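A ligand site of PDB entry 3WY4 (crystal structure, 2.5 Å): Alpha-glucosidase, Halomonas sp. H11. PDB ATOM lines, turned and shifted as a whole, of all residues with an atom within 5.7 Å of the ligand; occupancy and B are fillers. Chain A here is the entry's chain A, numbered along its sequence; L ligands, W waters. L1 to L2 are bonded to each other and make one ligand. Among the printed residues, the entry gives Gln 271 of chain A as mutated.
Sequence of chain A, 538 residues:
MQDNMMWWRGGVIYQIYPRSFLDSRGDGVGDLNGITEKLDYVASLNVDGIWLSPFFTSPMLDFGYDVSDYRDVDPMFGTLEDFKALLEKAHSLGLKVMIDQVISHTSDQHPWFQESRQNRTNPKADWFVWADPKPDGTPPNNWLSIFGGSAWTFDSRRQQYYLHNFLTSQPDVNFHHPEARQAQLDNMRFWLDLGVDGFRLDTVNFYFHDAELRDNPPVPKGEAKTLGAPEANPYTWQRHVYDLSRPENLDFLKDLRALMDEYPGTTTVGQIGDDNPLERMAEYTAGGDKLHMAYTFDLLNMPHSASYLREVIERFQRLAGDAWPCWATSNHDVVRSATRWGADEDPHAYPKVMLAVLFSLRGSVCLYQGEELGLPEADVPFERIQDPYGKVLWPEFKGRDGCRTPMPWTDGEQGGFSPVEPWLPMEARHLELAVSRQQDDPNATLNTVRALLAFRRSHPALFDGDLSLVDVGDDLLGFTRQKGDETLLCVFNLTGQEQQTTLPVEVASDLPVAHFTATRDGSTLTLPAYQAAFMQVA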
ATOM      1  N   ASP A  62      18.987  16.324 -13.911  1.00  0.00           N
ATOM      2  CA  ASP A  62      18.213  15.090 -13.923  1.00  0.00           C
ATOM      3  C   ASP A  62      17.538  14.930 -12.560  1.00  0.00           C
ATOM      4  O   ASP A  62      17.088  13.853 -12.187  1.00  0.00           O
ATOM      5  CB  ASP A  62      19.114  13.878 -14.222  1.00  0.00           C
ATOM      6  CG  ASP A  62      18.312  12.641 -14.598  1.00  0.00           C
ATOM      7  OD1 ASP A  62      17.113  12.775 -14.926  1.00  0.00           O
ATOM      8  OD2 ASP A  62      18.880  11.532 -14.545  1.00  0.00           O
ATOM      9  N   TYR A  65      19.842  12.732  -9.884  1.00  0.00           N
ATOM     10  CA  TYR A  65      20.655  11.664 -10.450  1.00  0.00           C
ATOM     11  C   TYR A  65      21.886  12.154 -11.206  1.00  0.00           C
ATOM     12  O   TYR A  65      22.600  11.369 -11.828  1.00  0.00           O
ATOM     13  CB  TYR A  65      19.798  10.744 -11.332  1.00  0.00           C
ATOM     14  CG  TYR A  65      18.812   9.913 -10.534  1.00  0.00           C
ATOM     15  CD1 TYR A  65      19.168   8.661 -10.054  1.00  0.00           C
ATOM     16  CD2 TYR A  65      17.545  10.388 -10.253  1.00  0.00           C
ATOM     17  CE1 TYR A  65      18.284   7.896  -9.316  1.00  0.00           C
ATOM     18  CE2 TYR A  65      16.642   9.626  -9.518  1.00  0.00           C
ATOM     19  CZ  TYR A  65      17.024   8.386  -9.062  1.00  0.00           C
ATOM     20  OH  TYR A  65      16.132   7.636  -8.325  1.00  0.00           O
ATOM     21  N   VAL A 102      24.088   6.677  -6.957  1.00  0.00           N
ATOM     22  CA  VAL A 102      24.251   6.899  -8.392  1.00  0.00           C
ATOM     23  C   VAL A 102      25.744   6.924  -8.750  1.00  0.00           C
ATOM     24  O   VAL A 102      26.320   7.993  -8.953  1.00  0.00           O
ATOM     25  CB  VAL A 102      23.601   8.236  -8.802  1.00  0.00           C
ATOM     26  CG1 VAL A 102      23.503   8.346 -10.325  1.00  0.00           C
ATOM     27  CG2 VAL A 102      22.215   8.365  -8.178  1.00  0.00           C
ATOM     28  N   HIS A 105      27.453   7.178 -13.027  1.00  0.00           N
ATOM     29  CA  HIS A 105      27.751   8.445 -13.683  1.00  0.00           C
ATOM     30  C   HIS A 105      27.640   9.610 -12.702  1.00  0.00           C
ATOM     31  O   HIS A 105      26.837   9.574 -11.777  1.00  0.00           O
ATOM     32  CB  HIS A 105      26.822   8.666 -14.875  1.00  0.00           C
ATOM     33  CG  HIS A 105      25.379   8.478 -14.558  1.00  0.00           C
ATOM     34  ND1 HIS A 105      24.689   7.318 -14.841  1.00  0.00           N
ATOM     35  CD2 HIS A 105      24.472   9.302 -13.972  1.00  0.00           C
ATOM     36  CE1 HIS A 105      23.438   7.433 -14.448  1.00  0.00           C
ATOM     37  NE2 HIS A 105      23.278   8.632 -13.918  1.00  0.00           N
ATOM     38  N   ILE A 146      19.919   7.359 -23.773  1.00  0.00           N
ATOM     39  CA  ILE A 146      18.519   7.101 -23.473  1.00  0.00           C
ATOM     40  C   ILE A 146      17.703   8.391 -23.516  1.00  0.00           C
ATOM     41  O   ILE A 146      16.537   8.389 -23.937  1.00  0.00           O
ATOM     42  CB  ILE A 146      18.361   6.415 -22.103  1.00  0.00           C
ATOM     43  CG1 ILE A 146      19.167   5.119 -22.068  1.00  0.00           C
ATOM     44  CG2 ILE A 146      16.896   6.145 -21.792  1.00  0.00           C
ATOM     45  CD1 ILE A 146      19.080   4.369 -20.760  1.00  0.00           C
ATOM     46  N   PHE A 147      18.311   9.484 -23.104  1.00  0.00           N
ATOM     47  CA  PHE A 147      17.637  10.777 -23.068  1.00  0.00           C
ATOM     48  C   PHE A 147      17.748  11.545 -24.379  1.00  0.00           C
ATOM     49  O   PHE A 147      17.409  12.720 -24.450  1.00  0.00           O
ATOM     50  CB  PHE A 147      18.163  11.624 -21.904  1.00  0.00           C
ATOM     51  CG  PHE A 147      17.823  11.068 -20.543  1.00  0.00           C
ATOM     52  CD1 PHE A 147      16.762  10.192 -20.382  1.00  0.00           C
ATOM     53  CD2 PHE A 147      18.553  11.435 -19.427  1.00  0.00           C
ATOM     54  CE1 PHE A 147      16.449   9.681 -19.145  1.00  0.00           C
ATOM     55  CE2 PHE A 147      18.240  10.931 -18.183  1.00  0.00           C
ATOM     56  CZ  PHE A 147      17.181  10.049 -18.043  1.00  0.00           C
ATOM     57  N   PHE A 166      23.083   8.756 -20.505  1.00  0.00           N
ATOM     58  CA  PHE A 166      21.938   9.629 -20.249  1.00  0.00           C
ATOM     59  C   PHE A 166      22.231  11.051 -20.707  1.00  0.00           C
ATOM     60  O   PHE A 166      22.644  11.267 -21.838  1.00  0.00           O
ATOM     61  CB  PHE A 166      21.549   9.575 -18.765  1.00  0.00           C
ATOM     62  CG  PHE A 166      21.206   8.189 -18.285  1.00  0.00           C
ATOM     63  CD1 PHE A 166      19.914   7.708 -18.391  1.00  0.00           C
ATOM     64  CD2 PHE A 166      22.186   7.373 -17.728  1.00  0.00           C
ATOM     65  CE1 PHE A 166      19.598   6.442 -17.953  1.00  0.00           C
ATOM     66  CE2 PHE A 166      21.870   6.107 -17.290  1.00  0.00           C
ATOM     67  CZ  PHE A 166      20.580   5.633 -17.402  1.00  0.00           C
ATOM     68  N   GLN A 170      25.785  14.174 -17.728  1.00  0.00           N
ATOM     69  CA  GLN A 170      25.956  12.982 -16.910  1.00  0.00           C
ATOM     70  C   GLN A 170      26.997  12.030 -17.501  1.00  0.00           C
ATOM     71  O   GLN A 170      26.646  10.951 -17.979  1.00  0.00           O
ATOM     72  CB  GLN A 170      24.622  12.255 -16.737  1.00  0.00           C
ATOM     73  CG  GLN A 170      23.663  12.929 -15.770  1.00  0.00           C
ATOM     74  CD  GLN A 170      22.298  12.265 -15.735  1.00  0.00           C
ATOM     75  OE1 GLN A 170      21.665  12.072 -16.766  1.00  0.00           O
ATOM     76  NE2 GLN A 170      21.850  11.900 -14.536  1.00  0.00           N
ATOM     77  N   ARG A 200      19.758   1.676  -2.779  1.00  0.00           N
ATOM     78  CA  ARG A 200      19.167   1.370  -4.071  1.00  0.00           C
ATOM     79  C   ARG A 200      20.212   1.705  -5.120  1.00  0.00           C
ATOM     80  O   ARG A 200      20.591   2.866  -5.272  1.00  0.00           O
ATOM     81  CB  ARG A 200      17.889   2.177  -4.297  1.00  0.00           C
ATOM     82  CG  ARG A 200      17.185   1.897  -5.628  1.00  0.00           C
ATOM     83  CD  ARG A 200      17.633   2.858  -6.721  1.00  0.00           C
ATOM     84  NE  ARG A 200      16.787   2.779  -7.910  1.00  0.00           N
ATOM     85  CZ  ARG A 200      16.916   3.573  -8.974  1.00  0.00           C
ATOM     86  NH1 ARG A 200      17.851   4.511  -8.988  1.00  0.00           N
ATOM     87  NH2 ARG A 200      16.097   3.431 -10.010  1.00  0.00           N
ATOM     88  N   ASP A 202      21.445   2.596  -8.477  1.00  0.00           N
ATOM     89  CA  ASP A 202      20.995   3.196  -9.717  1.00  0.00           C
ATOM     90  C   ASP A 202      21.744   2.648 -10.921  1.00  0.00           C
ATOM     91  O   ASP A 202      22.976   2.643 -10.941  1.00  0.00           O
ATOM     92  CB  ASP A 202      21.161   4.708  -9.648  1.00  0.00           C
ATOM     93  CG  ASP A 202      20.656   5.403 -10.894  1.00  0.00           C
ATOM     94  OD1 ASP A 202      19.432   5.454 -11.078  1.00  0.00           O
ATOM     95  OD2 ASP A 202      21.493   5.906 -11.676  1.00  0.00           O
ATOM     96  N   THR A 203      20.993   2.192 -11.928  1.00  0.00           N
ATOM     97  CA  THR A 203      21.562   1.644 -13.160  1.00  0.00           C
ATOM     98  C   THR A 203      22.651   0.619 -12.872  1.00  0.00           C
ATOM     99  O   THR A 203      23.772   0.739 -13.371  1.00  0.00           O
ATOM    100  CB  THR A 203      22.148   2.759 -14.055  1.00  0.00           C
ATOM    101  OG1 THR A 203      23.341   3.270 -13.463  1.00  0.00           O
ATOM    102  CG2 THR A 203      21.151   3.891 -14.225  1.00  0.00           C
ATOM    103  N   PHE A 206      24.716  -1.017 -15.544  1.00  0.00           N
ATOM    104  CA  PHE A 206      25.329  -0.071 -16.461  1.00  0.00           C
ATOM    105  C   PHE A 206      26.802   0.191 -16.155  1.00  0.00           C
ATOM    106  O   PHE A 206      27.478   0.834 -16.944  1.00  0.00           O
ATOM    107  CB  PHE A 206      24.572   1.258 -16.444  1.00  0.00           C
ATOM    108  CG  PHE A 206      23.329   1.270 -17.284  1.00  0.00           C
ATOM    109  CD1 PHE A 206      23.299   1.975 -18.483  1.00  0.00           C
ATOM    110  CD2 PHE A 206      22.200   0.577 -16.884  1.00  0.00           C
ATOM    111  CE1 PHE A 206      22.159   1.989 -19.257  1.00  0.00           C
ATOM    112  CE2 PHE A 206      21.060   0.585 -17.665  1.00  0.00           C
ATOM    113  CZ  PHE A 206      21.041   1.301 -18.848  1.00  0.00           C
ATOM    114  N   GLY A 228      12.579  -0.823 -20.692  1.00  0.00           N
ATOM    115  CA  GLY A 228      13.093   0.309 -19.950  1.00  0.00           C
ATOM    116  C   GLY A 228      13.003   1.634 -20.687  1.00  0.00           C
ATOM    117  O   GLY A 228      13.551   2.641 -20.237  1.00  0.00           O
ATOM    118  N   ALA A 229      12.304   1.636 -21.814  1.00  0.00           N
ATOM    119  CA  ALA A 229      12.174   2.835 -22.626  1.00  0.00           C
ATOM    120  C   ALA A 229      10.872   2.827 -23.434  1.00  0.00           C
ATOM    121  O   ALA A 229      10.370   1.757 -23.785  1.00  0.00           O
ATOM    122  CB  ALA A 229      13.373   2.968 -23.557  1.00  0.00           C
ATOM    123  N   GLN A 271      18.675  -1.509  -9.731  1.00  0.00           N
ATOM    124  CA  GLN A 271      17.741  -1.202 -10.800  1.00  0.00           C
ATOM    125  C   GLN A 271      18.259  -1.772 -12.119  1.00  0.00           C
ATOM    126  O   GLN A 271      19.290  -1.330 -12.629  1.00  0.00           O
ATOM    127  CB  GLN A 271      17.538   0.300 -10.940  1.00  0.00           C
ATOM    128  CG  GLN A 271      16.484   0.680 -11.953  1.00  0.00           C
ATOM    129  CD  GLN A 271      16.839   1.952 -12.707  1.00  0.00           C
ATOM    130  OE1 GLN A 271      18.009   2.228 -12.957  1.00  0.00           O
ATOM    131  NE2 GLN A 271      15.824   2.726 -13.078  1.00  0.00           N
ATOM    132  N   ILE A 272      17.544  -2.755 -12.659  1.00  0.00           N
ATOM    133  CA  ILE A 272      17.970  -3.418 -13.881  1.00  0.00           C
ATOM    134  C   ILE A 272      17.349  -2.791 -15.119  1.00  0.00           C
ATOM    135  O   ILE A 272      16.137  -2.654 -15.220  1.00  0.00           O
ATOM    136  CB  ILE A 272      17.615  -4.920 -13.851  1.00  0.00           C
ATOM    137  CG1 ILE A 272      18.251  -5.611 -12.649  1.00  0.00           C
ATOM    138  CG2 ILE A 272      18.060  -5.595 -15.143  1.00  0.00           C
ATOM    139  CD1 ILE A 272      19.757  -5.789 -12.768  1.00  0.00           C
ATOM    140  N   GLY A 273      18.213  -2.411 -16.073  1.00  0.00           N
ATOM    141  CA  GLY A 273      17.762  -1.930 -17.367  1.00  0.00           C
ATOM    142  C   GLY A 273      18.453  -2.727 -18.452  1.00  0.00           C
ATOM    143  O   GLY A 273      19.550  -2.378 -18.890  1.00  0.00           O
ATOM    144  N   ASP A 274      17.801  -3.797 -18.899  1.00  0.00           N
ATOM    145  CA  ASP A 274      18.454  -4.765 -19.787  1.00  0.00           C
ATOM    146  C   ASP A 274      17.465  -5.355 -20.794  1.00  0.00           C
ATOM    147  O   ASP A 274      16.261  -5.360 -20.562  1.00  0.00           O
ATOM    148  CB  ASP A 274      19.087  -5.872 -18.951  1.00  0.00           C
ATOM    149  CG  ASP A 274      19.971  -6.801 -19.766  1.00  0.00           C
ATOM    150  OD1 ASP A 274      21.150  -6.448 -19.990  1.00  0.00           O
ATOM    151  OD2 ASP A 274      19.478  -7.869 -20.173  1.00  0.00           O
ATOM    152  N   TYR A 295      15.158  -5.059  -9.044  1.00  0.00           N
ATOM    153  CA  TYR A 295      13.855  -4.939  -9.711  1.00  0.00           C
ATOM    154  C   TYR A 295      14.003  -4.590 -11.181  1.00  0.00           C
ATOM    155  O   TYR A 295      14.995  -3.997 -11.599  1.00  0.00           O
ATOM    156  CB  TYR A 295      12.947  -3.936  -8.991  1.00  0.00           C
ATOM    157  CG  TYR A 295      13.307  -2.483  -9.179  1.00  0.00           C
ATOM    158  CD1 TYR A 295      12.748  -1.741 -10.224  1.00  0.00           C
ATOM    159  CD2 TYR A 295      14.174  -1.830  -8.312  1.00  0.00           C
ATOM    160  CE1 TYR A 295      13.064  -0.411 -10.395  1.00  0.00           C
ATOM    161  CE2 TYR A 295      14.490  -0.493  -8.475  1.00  0.00           C
ATOM    162  CZ  TYR A 295      13.925   0.207  -9.522  1.00  0.00           C
ATOM    163  OH  TYR A 295      14.241   1.537  -9.693  1.00  0.00           O
ATOM    164  N   PHE A 297      11.710  -3.828 -15.213  1.00  0.00           N
ATOM    165  CA  PHE A 297      10.602  -3.084 -15.815  1.00  0.00           C
ATOM    166  C   PHE A 297       9.471  -4.008 -16.246  1.00  0.00           C
ATOM    167  O   PHE A 297       8.538  -3.580 -16.924  1.00  0.00           O
ATOM    168  CB  PHE A 297      11.093  -2.280 -17.022  1.00  0.00           C
ATOM    169  CG  PHE A 297      11.782  -0.996 -16.662  1.00  0.00           C
ATOM    170  CD1 PHE A 297      11.083   0.194 -16.640  1.00  0.00           C
ATOM    171  CD2 PHE A 297      13.128  -0.988 -16.342  1.00  0.00           C
ATOM    172  CE1 PHE A 297      11.708   1.381 -16.301  1.00  0.00           C
ATOM    173  CE2 PHE A 297      13.764   0.191 -16.009  1.00  0.00           C
ATOM    174  CZ  PHE A 297      13.055   1.383 -15.988  1.00  0.00           C
ATOM    175  N   HIS A 332       9.543   6.542  -9.847  1.00  0.00           N
ATOM    176  CA  HIS A 332       9.731   7.897 -10.352  1.00  0.00           C
ATOM    177  C   HIS A 332      10.076   7.929 -11.844  1.00  0.00           C
ATOM    178  O   HIS A 332      10.375   8.990 -12.392  1.00  0.00           O
ATOM    179  CB  HIS A 332      10.833   8.597  -9.568  1.00  0.00           C
ATOM    180  CG  HIS A 332      12.177   7.967  -9.720  1.00  0.00           C
ATOM    181  ND1 HIS A 332      12.438   6.671  -9.335  1.00  0.00           N
ATOM    182  CD2 HIS A 332      13.339   8.447 -10.237  1.00  0.00           C
ATOM    183  CE1 HIS A 332      13.704   6.383  -9.610  1.00  0.00           C
ATOM    184  NE2 HIS A 332      14.267   7.444 -10.145  1.00  0.00           N
ATOM    185  N   ASP A 333      10.025   6.770 -12.492  1.00  0.00           N
ATOM    186  CA  ASP A 333      10.418   6.676 -13.894  1.00  0.00           C
ATOM    187  C   ASP A 333       9.286   6.275 -14.831  1.00  0.00           C
ATOM    188  O   ASP A 333       9.403   6.420 -16.047  1.00  0.00           O
ATOM    189  CB  ASP A 333      11.585   5.694 -14.065  1.00  0.00           C
ATOM    190  CG  ASP A 333      12.876   6.220 -13.500  1.00  0.00           C
ATOM    191  OD1 ASP A 333      13.119   7.434 -13.578  1.00  0.00           O
ATOM    192  OD2 ASP A 333      13.654   5.408 -12.959  1.00  0.00           O
ATOM    193  N   TYR A 389      13.763  14.730 -20.010  1.00  0.00           N
ATOM    194  CA  TYR A 389      13.349  13.563 -20.774  1.00  0.00           C
ATOM    195  C   TYR A 389      11.978  13.799 -21.412  1.00  0.00           C
ATOM    196  O   TYR A 389      11.566  13.076 -22.310  1.00  0.00           O
ATOM    197  CB  TYR A 389      13.304  12.327 -19.862  1.00  0.00           C
ATOM    198  CG  TYR A 389      13.347  10.993 -20.580  1.00  0.00           C
ATOM    199  CD1 TYR A 389      13.663  10.914 -21.929  1.00  0.00           C
ATOM    200  CD2 TYR A 389      13.050   9.817 -19.899  1.00  0.00           C
ATOM    201  CE1 TYR A 389      13.706   9.698 -22.579  1.00  0.00           C
ATOM    202  CE2 TYR A 389      13.083   8.602 -20.550  1.00  0.00           C
ATOM    203  CZ  TYR A 389      13.411   8.543 -21.890  1.00  0.00           C
ATOM    204  OH  TYR A 389      13.441   7.327 -22.527  1.00  0.00           O
ATOM    205  N   ARG A 400       8.566  12.050 -17.318  1.00  0.00           N
ATOM    206  CA  ARG A 400       8.241  11.335 -16.096  1.00  0.00           C
ATOM    207  C   ARG A 400       7.629  12.228 -15.017  1.00  0.00           C
ATOM    208  O   ARG A 400       7.385  11.779 -13.903  1.00  0.00           O
ATOM    209  CB  ARG A 400       9.488  10.636 -15.550  1.00  0.00           C
ATOM    210  CG  ARG A 400      10.118   9.641 -16.522  1.00  0.00           C
ATOM    211  CD  ARG A 400      11.563   9.359 -16.153  1.00  0.00           C
ATOM    212  NE  ARG A 400      12.416  10.533 -16.316  1.00  0.00           N
ATOM    213  CZ  ARG A 400      13.713  10.559 -16.053  1.00  0.00           C
ATOM    214  NH1 ARG A 400      14.328   9.471 -15.612  1.00  0.00           N
ATOM    215  NH2 ARG A 400      14.407  11.674 -16.243  1.00  0.00           N
ATOM    216  N   ARG A 404       5.662  12.442 -10.694  1.00  0.00           N
ATOM    217  CA  ARG A 404       6.514  13.181  -9.768  1.00  0.00           C
ATOM    218  C   ARG A 404       5.843  14.452  -9.238  1.00  0.00           C
ATOM    219  O   ARG A 404       6.512  15.311  -8.667  1.00  0.00           O
ATOM    220  CB  ARG A 404       7.871  13.493 -10.403  1.00  0.00           C
ATOM    221  CG  ARG A 404       8.863  12.350 -10.277  1.00  0.00           C
ATOM    222  CD  ARG A 404       9.510  11.996 -11.605  1.00  0.00           C
ATOM    223  NE  ARG A 404      10.581  12.919 -11.985  1.00  0.00           N
ATOM    224  CZ  ARG A 404      11.699  12.544 -12.602  1.00  0.00           C
ATOM    225  NH1 ARG A 404      11.886  11.272 -12.915  1.00  0.00           N
ATOM    226  NH2 ARG A 404      12.621  13.437 -12.914  1.00  0.00           N
HETATM  227  C1  LIG L   1      16.365   3.360 -18.559  1.00  0.00           C
HETATM  228  C2  LIG L   1      17.454   2.794 -17.646  1.00  0.00           C
HETATM  229  C3  LIG L   1      17.248   3.200 -16.190  1.00  0.00           C
HETATM  230  C4  LIG L   1      16.998   4.703 -16.086  1.00  0.00           C
HETATM  231  C5  LIG L   1      15.862   5.085 -17.034  1.00  0.00           C
HETATM  232  C6  LIG L   1      15.525   6.558 -16.930  1.00  0.00           C
HETATM  233  O1  LIG L   1      15.134   2.726 -18.294  1.00  0.00           O
HETATM  234  O2  LIG L   1      17.451   1.380 -17.736  1.00  0.00           O
HETATM  235  O3  LIG L   1      18.399   2.842 -15.454  1.00  0.00           O
HETATM  236  O4  LIG L   1      16.644   5.083 -14.768  1.00  0.00           O
HETATM  237  O5  LIG L   1      16.235   4.752 -18.354  1.00  0.00           O
HETATM  238  O6  LIG L   1      14.432   6.856 -17.774  1.00  0.00           O
HETATM  239  C1  LG2 L   2      17.635   5.498 -13.832  1.00  0.00           C
HETATM  240  C2  LG2 L   2      16.981   6.333 -12.740  1.00  0.00           C
HETATM  241  C3  LG2 L   2      16.413   7.597 -13.368  1.00  0.00           C
HETATM  242  C4  LG2 L   2      17.574   8.402 -13.924  1.00  0.00           C
HETATM  243  C5  LG2 L   2      18.495   7.572 -14.816  1.00  0.00           C
HETATM  244  C6  LG2 L   2      19.865   8.243 -14.871  1.00  0.00           C
HETATM  245  O1  LG2 L   2      15.979   5.597 -12.070  1.00  0.00           O
HETATM  246  O2  LG2 L   2      15.734   8.350 -12.404  1.00  0.00           O
HETATM  247  O3  LG2 L   2      17.066   9.471 -14.685  1.00  0.00           O
HETATM  248  O4  LG2 L   2      18.702   6.225 -14.398  1.00  0.00           O
HETATM  249  O5  LG2 L   2      20.412   8.291 -13.572  1.00  0.00           O
HETATM  250  O   HOH W   1      16.482  -0.408 -20.033  1.00  0.00           O
HETATM  251  O   HOH W   2      13.344   5.335 -20.410  1.00  0.00           O
HETATM  252  O   HOH W   3      15.275  11.351 -12.872  1.00  0.00           O
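Water W3 lies within hydrogen-bond range of an oxygen (O2) of LG2 L2 (3.1 Å), the side-chain carboxylate (OD1) of Asp 62 (3.1 Å), the guanidinium group (NH2) of Arg 404 (3.4 Å) and the guanidinium group (NH1) of Arg 400 (3.5 Å). Water W2 lies within hydrogen-bond range of O of Gly 228, OH of Tyr 389 and O6 of LIG L1.
OD2 of Asp 333 lies within hydrogen-bond range of O1 of LG2 L2, 2.5 Å away. An oxygen (O1) of LIG L1 lies within hydrogen-bond range of the backbone carbonyl oxygen (O) of Gly 228. An oxygen (O3) of LIG L1 sits at hydrogen-bond distance from the side-chain amide oxygen of Gln 271, 2.6 Å away. O3 of LG2 L2 sits at hydrogen-bond distance from OD2 of Asp 62, at 2.7 Å. NE2 of His 332 is in hydrogen-bond range of O2 of LG2 L2, 2.8 Å away. The guanidinium group (NH1) of Arg 400 lies within hydrogen-bond range of an oxygen (O3) of LG2 L2, 2.9 Å away. A ring nitrogen (NE2) of His 105 sits at hydrogen-bond distance from an oxygen (O5) of LG2 L2, 2.9 Å away. The guanidinium group (NH2) of Arg 200 lies within hydrogen-bond range of an oxygen (O1) of LG2 L2 (3.0 Å). OD2 of Asp 202 is in hydrogen-bond range of O5 of LG2 L2 (3.2 Å).
OD1 of Asp 333 is in salt-bridge range of NH1 of Arg 400 (3.1 Å). The guanidinium group (NH2) of Arg 200 sits close to the side-chain amide nitrogen (NE2) of Gln 271. The side-chain carboxylate (OD1) of Asp 62 lies within salt-bridge range of the guanidinium group (NH2) of Arg 400, at 3.2 Å. OD2 of Asp 62 is in hydrogen-bond range of NE2 of Gln 170. The side-chain hydroxyl (OH) of Tyr 65 sits at hydrogen-bond distance from a ring nitrogen (NE2) of His 332, 2.6 Å away. NH1 of Arg 200 is in salt-bridge range of OD1 of Asp 202 (2.8 Å). The guanidinium group of Arg 200 sits at hydrogen-bond distance from the side-chain hydroxyl of Tyr 295 (2.7 Å). O of Tyr 65 is in hydrogen-bond range of NE2 of Gln 170.
CE2 of Tyr 65 touches O2 of LG2 L2 (3.3 Å). CD1 of Ile 146 touches C1 of LIG L1 (3.6 Å). CZ of Phe 147 touches O3 of LG2 L2 (3.4 Å). Phe 166 touches the ligand. Thr 203 touches the ligand. CE2 of Phe 206 touches O2 of LIG L1, 3.7 Å away. Gly 273 touches the ligand. CZ of Phe 297 touches O1 of LIG L1 (3.4 Å). CE2 of Tyr 389 touches O6 of LIG L1 (3.5 Å). Hydrophobic or aromatic side chains within 4 Å of the ligand: Tyr 65, His 105, Ile 146, Phe 147, Phe 166, Phe 206, Phe 297, His 332 and Tyr 389. Of the 25 residues printed, 18 come within 4 Å of the ligand.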
